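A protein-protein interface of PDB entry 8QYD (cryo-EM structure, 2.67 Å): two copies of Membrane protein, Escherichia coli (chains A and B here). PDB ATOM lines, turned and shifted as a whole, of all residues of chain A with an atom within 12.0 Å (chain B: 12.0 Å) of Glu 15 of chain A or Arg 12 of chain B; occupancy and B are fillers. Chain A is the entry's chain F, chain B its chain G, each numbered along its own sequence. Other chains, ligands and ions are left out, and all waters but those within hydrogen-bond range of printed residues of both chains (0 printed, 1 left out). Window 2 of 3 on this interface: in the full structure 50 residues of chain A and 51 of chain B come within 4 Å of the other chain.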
ATOM      1  N   VAL A   8      -2.150 -31.750  -5.675  1.00  0.00           N
ATOM      2  CA  VAL A   8      -1.897 -30.337  -5.424  1.00  0.00           C
ATOM      3  C   VAL A   8      -3.135 -29.519  -5.775  1.00  0.00           C
ATOM      4  O   VAL A   8      -3.889 -29.844  -6.703  1.00  0.00           O
ATOM      5  CB  VAL A   8      -0.664 -29.855  -6.212  1.00  0.00           C
ATOM      6  CG1 VAL A   8       0.549 -30.711  -5.874  1.00  0.00           C
ATOM      7  CG2 VAL A   8      -0.935 -29.885  -7.710  1.00  0.00           C
ATOM      8  N   LYS A   9      -3.358 -28.453  -5.011  1.00  0.00           N
ATOM      9  CA  LYS A   9      -4.510 -27.584  -5.197  1.00  0.00           C
ATOM     10  C   LYS A   9      -4.032 -26.138  -5.128  1.00  0.00           C
ATOM     11  O   LYS A   9      -2.830 -25.864  -5.053  1.00  0.00           O
ATOM     12  CB  LYS A   9      -5.595 -27.890  -4.155  1.00  0.00           C
ATOM     13  CG  LYS A   9      -6.801 -28.632  -4.704  1.00  0.00           C
ATOM     14  CD  LYS A   9      -6.533 -30.120  -4.838  1.00  0.00           C
ATOM     15  CE  LYS A   9      -7.687 -30.825  -5.534  1.00  0.00           C
ATOM     16  NZ  LYS A   9      -7.414 -32.275  -5.736  1.00  0.00           N
ATOM     17  N   LYS A  10      -4.990 -25.208  -5.170  1.00  0.00           N
ATOM     18  CA  LYS A  10      -4.727 -23.772  -5.056  1.00  0.00           C
ATOM     19  C   LYS A  10      -3.783 -23.281  -6.153  1.00  0.00           C
ATOM     20  O   LYS A  10      -3.077 -22.284  -5.986  1.00  0.00           O
ATOM     21  CB  LYS A  10      -4.177 -23.421  -3.667  1.00  0.00           C
ATOM     22  CG  LYS A  10      -4.360 -21.964  -3.249  1.00  0.00           C
ATOM     23  CD  LYS A  10      -3.178 -21.458  -2.434  1.00  0.00           C
ATOM     24  CE  LYS A  10      -1.929 -21.319  -3.290  1.00  0.00           C
ATOM     25  NZ  LYS A  10      -0.898 -20.459  -2.656  1.00  0.00           N
ATOM     26  N   ARG A  11      -3.768 -23.963  -7.296  1.00  0.00           N
ATOM     27  CA  ARG A  11      -2.920 -23.538  -8.401  1.00  0.00           C
ATOM     28  C   ARG A  11      -3.528 -22.302  -9.050  1.00  0.00           C
ATOM     29  O   ARG A  11      -4.114 -22.380 -10.135  1.00  0.00           O
ATOM     30  CB  ARG A  11      -2.750 -24.672  -9.413  1.00  0.00           C
ATOM     31  CG  ARG A  11      -1.734 -24.398 -10.509  1.00  0.00           C
ATOM     32  CD  ARG A  11      -1.867 -25.413 -11.631  1.00  0.00           C
ATOM     33  NE  ARG A  11      -1.754 -26.779 -11.133  1.00  0.00           N
ATOM     34  CZ  ARG A  11      -2.304 -27.835 -11.715  1.00  0.00           C
ATOM     35  NH1 ARG A  11      -3.022 -27.720 -12.820  1.00  0.00           N
ATOM     36  NH2 ARG A  11      -2.132 -29.037 -11.172  1.00  0.00           N
ATOM     37  N   ARG A  12      -3.401 -21.157  -8.381  1.00  0.00           N
ATOM     38  CA  ARG A  12      -4.091 -19.930  -8.782  1.00  0.00           C
ATOM     39  C   ARG A  12      -3.203 -18.747  -8.409  1.00  0.00           C
ATOM     40  O   ARG A  12      -3.165 -18.334  -7.246  1.00  0.00           O
ATOM     41  CB  ARG A  12      -5.463 -19.846  -8.117  1.00  0.00           C
ATOM     42  CG  ARG A  12      -6.348 -18.687  -8.562  1.00  0.00           C
ATOM     43  CD  ARG A  12      -6.187 -17.466  -7.666  1.00  0.00           C
ATOM     44  NE  ARG A  12      -7.142 -16.414  -7.995  1.00  0.00           N
ATOM     45  CZ  ARG A  12      -7.113 -15.191  -7.482  1.00  0.00           C
ATOM     46  NH1 ARG A  12      -6.194 -14.833  -6.601  1.00  0.00           N
ATOM     47  NH2 ARG A  12      -8.033 -14.309  -7.858  1.00  0.00           N
ATOM     48  N   SER A  13      -2.483 -18.217  -9.391  1.00  0.00           N
ATOM     49  CA  SER A  13      -1.687 -17.019  -9.170  1.00  0.00           C
ATOM     50  C   SER A  13      -2.597 -15.800  -9.103  1.00  0.00           C
ATOM     51  O   SER A  13      -3.485 -15.628  -9.944  1.00  0.00           O
ATOM     52  CB  SER A  13      -0.651 -16.854 -10.282  1.00  0.00           C
ATOM     53  OG  SER A  13      -1.275 -16.739 -11.550  1.00  0.00           O
ATOM     54  N   ASP A  14      -2.380 -14.958  -8.098  1.00  0.00           N
ATOM     55  CA  ASP A  14      -3.226 -13.789  -7.910  1.00  0.00           C
ATOM     56  C   ASP A  14      -3.005 -12.775  -9.025  1.00  0.00           C
ATOM     57  O   ASP A  14      -1.876 -12.548  -9.468  1.00  0.00           O
ATOM     58  CB  ASP A  14      -2.946 -13.150  -6.553  1.00  0.00           C
ATOM     59  CG  ASP A  14      -3.153 -14.116  -5.406  1.00  0.00           C
ATOM     60  OD1 ASP A  14      -2.230 -14.905  -5.118  1.00  0.00           O
ATOM     61  OD2 ASP A  14      -4.241 -14.089  -4.795  1.00  0.00           O
ATOM     62  N   GLU A  15      -4.098 -12.173  -9.485  1.00  0.00           N
ATOM     63  CA  GLU A  15      -4.022 -11.154 -10.520  1.00  0.00           C
ATOM     64  C   GLU A  15      -3.510  -9.843  -9.942  1.00  0.00           C
ATOM     65  O   GLU A  15      -3.909  -9.427  -8.851  1.00  0.00           O
ATOM     66  CB  GLU A  15      -5.391 -10.939 -11.165  1.00  0.00           C
ATOM     67  CG  GLU A  15      -5.893 -12.136 -11.944  1.00  0.00           C
ATOM     68  CD  GLU A  15      -5.049 -12.422 -13.168  1.00  0.00           C
ATOM     69  OE1 GLU A  15      -4.507 -11.463 -13.755  1.00  0.00           O
ATOM     70  OE2 GLU A  15      -4.926 -13.606 -13.542  1.00  0.00           O
ATOM     71  N   ALA A  16      -2.625  -9.191 -10.687  1.00  0.00           N
ATOM     72  CA  ALA A  16      -2.064  -7.920 -10.259  1.00  0.00           C
ATOM     73  C   ALA A  16      -3.077  -6.799 -10.443  1.00  0.00           C
ATOM     74  O   ALA A  16      -3.904  -6.830 -11.358  1.00  0.00           O
ATOM     75  CB  ALA A  16      -0.793  -7.609 -11.044  1.00  0.00           C
ATOM     76  N   GLU A  17      -3.002  -5.805  -9.562  1.00  0.00           N
ATOM     77  CA  GLU A  17      -3.902  -4.661  -9.631  1.00  0.00           C
ATOM     78  C   GLU A  17      -3.667  -3.867 -10.909  1.00  0.00           C
ATOM     79  O   GLU A  17      -2.522  -3.634 -11.308  1.00  0.00           O
ATOM     80  CB  GLU A  17      -3.699  -3.769  -8.408  1.00  0.00           C
ATOM     81  CG  GLU A  17      -4.480  -2.471  -8.440  1.00  0.00           C
ATOM     82  CD  GLU A  17      -5.888  -2.620  -7.907  1.00  0.00           C
ATOM     83  OE1 GLU A  17      -6.305  -3.763  -7.627  1.00  0.00           O
ATOM     84  OE2 GLU A  17      -6.578  -1.589  -7.768  1.00  0.00           O
ATOM     85  N   LYS A  18      -4.753  -3.454 -11.549  1.00  0.00           N
ATOM     86  CA  LYS A  18      -4.656  -2.613 -12.734  1.00  0.00           C
ATOM     87  C   LYS A  18      -4.322  -1.191 -12.301  1.00  0.00           C
ATOM     88  O   LYS A  18      -5.109  -0.577 -11.571  1.00  0.00           O
ATOM     89  CB  LYS A  18      -5.965  -2.642 -13.510  1.00  0.00           C
ATOM     90  CG  LYS A  18      -6.377  -4.018 -13.993  1.00  0.00           C
ATOM     91  CD  LYS A  18      -5.455  -4.539 -15.069  1.00  0.00           C
ATOM     92  CE  LYS A  18      -5.886  -5.920 -15.520  1.00  0.00           C
ATOM     93  NZ  LYS A  18      -7.185  -5.875 -16.235  1.00  0.00           N
ATOM     94  N   PRO A  19      -3.196  -0.629 -12.724  1.00  0.00           N
ATOM     95  CA  PRO A  19      -2.700   0.593 -12.080  1.00  0.00           C
ATOM     96  C   PRO A  19      -3.068   1.896 -12.771  1.00  0.00           C
ATOM     97  O   PRO A  19      -2.815   2.972 -12.222  1.00  0.00           O
ATOM     98  CB  PRO A  19      -1.184   0.383 -12.102  1.00  0.00           C
ATOM     99  CG  PRO A  19      -0.942  -0.459 -13.329  1.00  0.00           C
ATOM    100  CD  PRO A  19      -2.219  -1.182 -13.677  1.00  0.00           C
ATOM    101  N   ILE A  22      -5.947   4.147 -11.463  1.00  0.00           N
ATOM    102  CA  ILE A  22      -5.425   4.761 -10.245  1.00  0.00           C
ATOM    103  C   ILE A  22      -4.596   5.991 -10.590  1.00  0.00           C
ATOM    104  O   ILE A  22      -4.726   7.051  -9.964  1.00  0.00           O
ATOM    105  CB  ILE A  22      -4.604   3.734  -9.445  1.00  0.00           C
ATOM    106  CG1 ILE A  22      -5.441   2.485  -9.164  1.00  0.00           C
ATOM    107  CG2 ILE A  22      -4.098   4.348  -8.155  1.00  0.00           C
ATOM    108  CD1 ILE A  22      -4.854   1.577  -8.113  1.00  0.00           C
ATOM    109  N   VAL B   8     -13.045 -30.952 -12.287  1.00  0.00           N
ATOM    110  CA  VAL B   8     -12.762 -29.776 -13.100  1.00  0.00           C
ATOM    111  C   VAL B   8     -12.320 -28.632 -12.202  1.00  0.00           C
ATOM    112  O   VAL B   8     -12.666 -28.568 -11.015  1.00  0.00           O
ATOM    113  CB  VAL B   8     -13.987 -29.376 -13.950  1.00  0.00           C
ATOM    114  CG1 VAL B   8     -14.180 -30.362 -15.089  1.00  0.00           C
ATOM    115  CG2 VAL B   8     -15.233 -29.307 -13.081  1.00  0.00           C
ATOM    116  N   LYS B   9     -11.540 -27.719 -12.775  1.00  0.00           N
ATOM    117  CA  LYS B   9     -11.045 -26.544 -12.076  1.00  0.00           C
ATOM    118  C   LYS B   9     -11.502 -25.292 -12.811  1.00  0.00           C
ATOM    119  O   LYS B   9     -11.554 -25.270 -14.046  1.00  0.00           O
ATOM    120  CB  LYS B   9      -9.514 -26.557 -11.967  1.00  0.00           C
ATOM    121  CG  LYS B   9      -8.958 -27.389 -10.814  1.00  0.00           C
ATOM    122  CD  LYS B   9      -9.064 -28.883 -11.090  1.00  0.00           C
ATOM    123  CE  LYS B   9      -8.116 -29.305 -12.204  1.00  0.00           C
ATOM    124  NZ  LYS B   9      -8.157 -30.773 -12.453  1.00  0.00           N
ATOM    125  N   LYS B  10     -11.837 -24.254 -12.049  1.00  0.00           N
ATOM    126  CA  LYS B  10     -12.289 -23.002 -12.634  1.00  0.00           C
ATOM    127  C   LYS B  10     -11.167 -22.359 -13.444  1.00  0.00           C
ATOM    128  O   LYS B  10      -9.983 -22.518 -13.140  1.00  0.00           O
ATOM    129  CB  LYS B  10     -12.757 -22.044 -11.538  1.00  0.00           C
ATOM    130  CG  LYS B  10     -13.931 -22.558 -10.719  1.00  0.00           C
ATOM    131  CD  LYS B  10     -15.162 -22.778 -11.576  1.00  0.00           C
ATOM    132  CE  LYS B  10     -15.710 -21.465 -12.106  1.00  0.00           C
ATOM    133  NZ  LYS B  10     -16.205 -20.586 -11.010  1.00  0.00           N
ATOM    134  N   ARG B  11     -11.550 -21.627 -14.490  1.00  0.00           N
ATOM    135  CA  ARG B  11     -10.544 -21.035 -15.356  1.00  0.00           C
ATOM    136  C   ARG B  11      -9.819 -19.897 -14.640  1.00  0.00           C
ATOM    137  O   ARG B  11     -10.136 -19.527 -13.506  1.00  0.00           O
ATOM    138  CB  ARG B  11     -11.155 -20.483 -16.645  1.00  0.00           C
ATOM    139  CG  ARG B  11     -12.100 -19.309 -16.436  1.00  0.00           C
ATOM    140  CD  ARG B  11     -12.638 -18.776 -17.759  1.00  0.00           C
ATOM    141  NE  ARG B  11     -13.471 -19.710 -18.506  1.00  0.00           N
ATOM    142  CZ  ARG B  11     -14.781 -19.833 -18.347  1.00  0.00           C
ATOM    143  NH1 ARG B  11     -15.441 -19.105 -17.461  1.00  0.00           N
ATOM    144  NH2 ARG B  11     -15.448 -20.691 -19.110  1.00  0.00           N
ATOM    145  N   ARG B  12      -8.830 -19.337 -15.332  1.00  0.00           N
ATOM    146  CA  ARG B  12      -8.164 -18.123 -14.881  1.00  0.00           C
ATOM    147  C   ARG B  12      -9.069 -16.928 -15.150  1.00  0.00           C
ATOM    148  O   ARG B  12      -8.956 -16.276 -16.194  1.00  0.00           O
ATOM    149  CB  ARG B  12      -6.814 -17.963 -15.587  1.00  0.00           C
ATOM    150  CG  ARG B  12      -6.038 -16.712 -15.211  1.00  0.00           C
ATOM    151  CD  ARG B  12      -5.611 -16.745 -13.759  1.00  0.00           C
ATOM    152  NE  ARG B  12      -4.658 -17.815 -13.499  1.00  0.00           N
ATOM    153  CZ  ARG B  12      -4.301 -18.218 -12.288  1.00  0.00           C
ATOM    154  NH1 ARG B  12      -4.793 -17.649 -11.200  1.00  0.00           N
ATOM    155  NH2 ARG B  12      -3.428 -19.213 -12.165  1.00  0.00           N
ATOM    156  N   SER B  13      -9.983 -16.645 -14.227  1.00  0.00           N
ATOM    157  CA  SER B  13     -10.974 -15.584 -14.397  1.00  0.00           C
ATOM    158  C   SER B  13     -10.437 -14.316 -13.745  1.00  0.00           C
ATOM    159  O   SER B  13     -10.597 -14.109 -12.540  1.00  0.00           O
ATOM    160  CB  SER B  13     -12.316 -15.994 -13.802  1.00  0.00           C
ATOM    161  OG  SER B  13     -12.191 -16.299 -12.424  1.00  0.00           O
ATOM    162  N   ASP B  14      -9.798 -13.467 -14.546  1.00  0.00           N
ATOM    163  CA  ASP B  14      -9.305 -12.197 -14.035  1.00  0.00           C
ATOM    164  C   ASP B  14     -10.472 -11.297 -13.654  1.00  0.00           C
ATOM    165  O   ASP B  14     -11.473 -11.209 -14.371  1.00  0.00           O
ATOM    166  CB  ASP B  14      -8.419 -11.508 -15.075  1.00  0.00           C
ATOM    167  CG  ASP B  14      -9.201 -11.015 -16.276  1.00  0.00           C
ATOM    168  OD1 ASP B  14     -10.041 -11.780 -16.792  1.00  0.00           O
ATOM    169  OD2 ASP B  14      -8.982  -9.861 -16.699  1.00  0.00           O
ATOM    170  N   GLU B  15     -10.346 -10.636 -12.511  1.00  0.00           N
ATOM    171  CA  GLU B  15     -11.425  -9.788 -12.041  1.00  0.00           C
ATOM    172  C   GLU B  15     -11.471  -8.493 -12.843  1.00  0.00           C
ATOM    173  O   GLU B  15     -10.511  -8.108 -13.516  1.00  0.00           O
ATOM    174  CB  GLU B  15     -11.271  -9.490 -10.550  1.00  0.00           C
ATOM    175  CG  GLU B  15     -11.939 -10.518  -9.647  1.00  0.00           C
ATOM    176  CD  GLU B  15     -13.435 -10.297  -9.501  1.00  0.00           C
ATOM    177  OE1 GLU B  15     -13.988  -9.434 -10.214  1.00  0.00           O
ATOM    178  OE2 GLU B  15     -14.060 -10.994  -8.674  1.00  0.00           O
ATOM    179  N   ALA B  16     -12.616  -7.824 -12.771  1.00  0.00           N
ATOM    180  CA  ALA B  16     -12.799  -6.580 -13.495  1.00  0.00           C
ATOM    181  C   ALA B  16     -12.062  -5.440 -12.802  1.00  0.00           C
ATOM    182  O   ALA B  16     -11.573  -5.569 -11.677  1.00  0.00           O
ATOM    183  CB  ALA B  16     -14.284  -6.246 -13.613  1.00  0.00           C
ATOM    184  N   GLU B  17     -11.979  -4.312 -13.502  1.00  0.00           N
ATOM    185  CA  GLU B  17     -11.477  -3.089 -12.893  1.00  0.00           C
ATOM    186  C   GLU B  17     -12.300  -2.748 -11.660  1.00  0.00           C
ATOM    187  O   GLU B  17     -13.529  -2.855 -11.666  1.00  0.00           O
ATOM    188  CB  GLU B  17     -11.539  -1.934 -13.893  1.00  0.00           C
ATOM    189  CG  GLU B  17     -10.373  -1.848 -14.857  1.00  0.00           C
ATOM    190  CD  GLU B  17      -9.201  -1.078 -14.285  1.00  0.00           C
ATOM    191  OE1 GLU B  17      -8.214  -0.862 -15.020  1.00  0.00           O
ATOM    192  OE2 GLU B  17      -9.266  -0.682 -13.103  1.00  0.00           O
ATOM    193  N   LYS B  18     -11.618  -2.347 -10.595  1.00  0.00           N
ATOM    194  CA  LYS B  18     -12.323  -1.932  -9.394  1.00  0.00           C
ATOM    195  C   LYS B  18     -13.123  -0.670  -9.696  1.00  0.00           C
ATOM    196  O   LYS B  18     -12.545   0.333 -10.136  1.00  0.00           O
ATOM    197  CB  LYS B  18     -11.345  -1.686  -8.249  1.00  0.00           C
ATOM    198  CG  LYS B  18     -10.331  -2.795  -8.069  1.00  0.00           C
ATOM    199  CD  LYS B  18      -9.445  -2.541  -6.866  1.00  0.00           C
ATOM    200  CE  LYS B  18     -10.240  -2.583  -5.574  1.00  0.00           C
ATOM    201  NZ  LYS B  18      -9.364  -2.396  -4.387  1.00  0.00           N
ATOM    202  N   TRP B  21     -12.054   3.185  -8.618  1.00  0.00           N
ATOM    203  CA  TRP B  21     -11.015   3.998  -9.238  1.00  0.00           C
ATOM    204  C   TRP B  21     -11.537   4.739 -10.462  1.00  0.00           C
ATOM    205  O   TRP B  21     -11.233   5.921 -10.651  1.00  0.00           O
ATOM    206  CB  TRP B  21      -9.818   3.126  -9.591  1.00  0.00           C
ATOM    207  CG  TRP B  21      -9.059   2.730  -8.382  1.00  0.00           C
ATOM    208  CD1 TRP B  21      -8.910   1.473  -7.884  1.00  0.00           C
ATOM    209  CD2 TRP B  21      -8.367   3.603  -7.488  1.00  0.00           C
ATOM    210  NE1 TRP B  21      -8.154   1.506  -6.741  1.00  0.00           N
ATOM    211  CE2 TRP B  21      -7.808   2.804  -6.476  1.00  0.00           C
ATOM    212  CE3 TRP B  21      -8.158   4.984  -7.450  1.00  0.00           C
ATOM    213  CZ2 TRP B  21      -7.055   3.338  -5.440  1.00  0.00           C
ATOM    214  CZ3 TRP B  21      -7.413   5.510  -6.422  1.00  0.00           C
ATOM    215  CH2 TRP B  21      -6.867   4.690  -5.433  1.00  0.00           C
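Printed residues of chain B within 4 Å of Arg 11 of chain A: Arg 12.
Arg 12 of chain A touches just one residue of chain B: Arg 12 (3.2 Å).
Ser 13 of chain A touches one residue of chain B.
No residue of chain B comes within 4 Å of Asp 14 of chain A.
Of chain B, only Arg 12 (3.2 Å) and Asp 14 (3.98 Å) come within 4 Å of Glu 15 of chain A.
Printed residues of chain B within 4 Å of Glu 17 of chain A: Lys 18 and Trp 21.
Pro 19 of chain A touches none of the printed residues of chain B.
Printed residues of chain B within 4 Å of Ile 22 of chain A: Trp 21.
Val 8 of chain B touches none of the printed residues of chain A.
No residue of chain A comes within 4 Å of Ser 13 of chain B.
Of chain A, only Glu 15 (3.98 Å) comes within 4 Å of Asp 14 of chain B.
Printed residues of chain A within 4 Å of Lys 18 of chain B: Glu 17 (3.2 Å).
Of the printed residues of chain A, Trp 21 of chain B touches Glu 17 and Ile 22.
The nearest residue of chain B that does not touch Glu 15 of chain A is Glu 15 of chain B (4.7 Å).
The nearest residue of chain A that does not touch Arg 12 of chain B is Asp 14 of chain A (4.8 Å).
The nearest printed residue of chain A that does not touch Trp 21 of chain B is Lys 18 of chain A (5.7 Å).
Of the 12 printed residues of chain B, 5 touch a printed residue of chain A.
Hydrophobic or aromatic side chains of chain B within 4 Å of the printed part of chain A: Trp 21.
Of the 13 printed residues of chain A, 7 touch a printed residue of chain B.
Printed residues of chain A that touch a printed residue of chain B: Arg 11, Arg 12, Ser 13, Glu 15, Glu 17, Lys 18 and Ile 22.
Hydrophobic or aromatic side chains of chain A that line the printed part of chain B: Ile 22.
Among the printed residues, no Asp or Glu carboxylate lies within 4 Å of a Lys or Arg side-chain nitrogen of the other chain.
The guanidinium group (NH1) of Arg 12 of chain B is in hydrogen-bond range of the backbone carbonyl oxygen (O) of Ser 13 of chain A (2.7 Å).
Arg 11 of chain A touches Arg 12 of chain B, but with the chains exchanged Arg 12 of chain A does not touch Arg 11 of chain B (6.3 Å).
Ser 13 of chain A touches Arg 12 of chain B, but with the chains exchanged Arg 12 of chain A does not touch Ser 13 of chain B (5.3 Å).
Glu 15 of chain A touches Arg 12 of chain B, but with the chains exchanged Arg 12 of chain A does not touch Glu 15 of chain B (5.7 Å).
Glu 15 of chain A touches Asp 14 of chain B, but with the chains exchanged Asp 14 of chain A does not touch Glu 15 of chain B (8.4 Å).
Of the 9 pairs that touch across the chains among the printed residues, 3 have their exchanged pair printed and touching as well.
NH1 of Arg 12 of chain A is in salt-bridge range of OD2 of Asp 14 of chain A (2.8 Å).
Among the printed residues, merely in contact across the chains: Arg 11 of chain A with Arg 12 of chain B, Arg 12 of chain A with Arg 12 of chain B, Glu 15 of chain A with Arg 12 of chain B, Glu 15 of chain A with Asp 14 of chain B, Glu 17 of chain A with Lys 18 of chain B, Glu 17 of chain A with Trp 21 of chain B, Lys 18 of chain A with Glu 17 of chain B and Ile 22 of chain A with Trp 21 of chain B.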
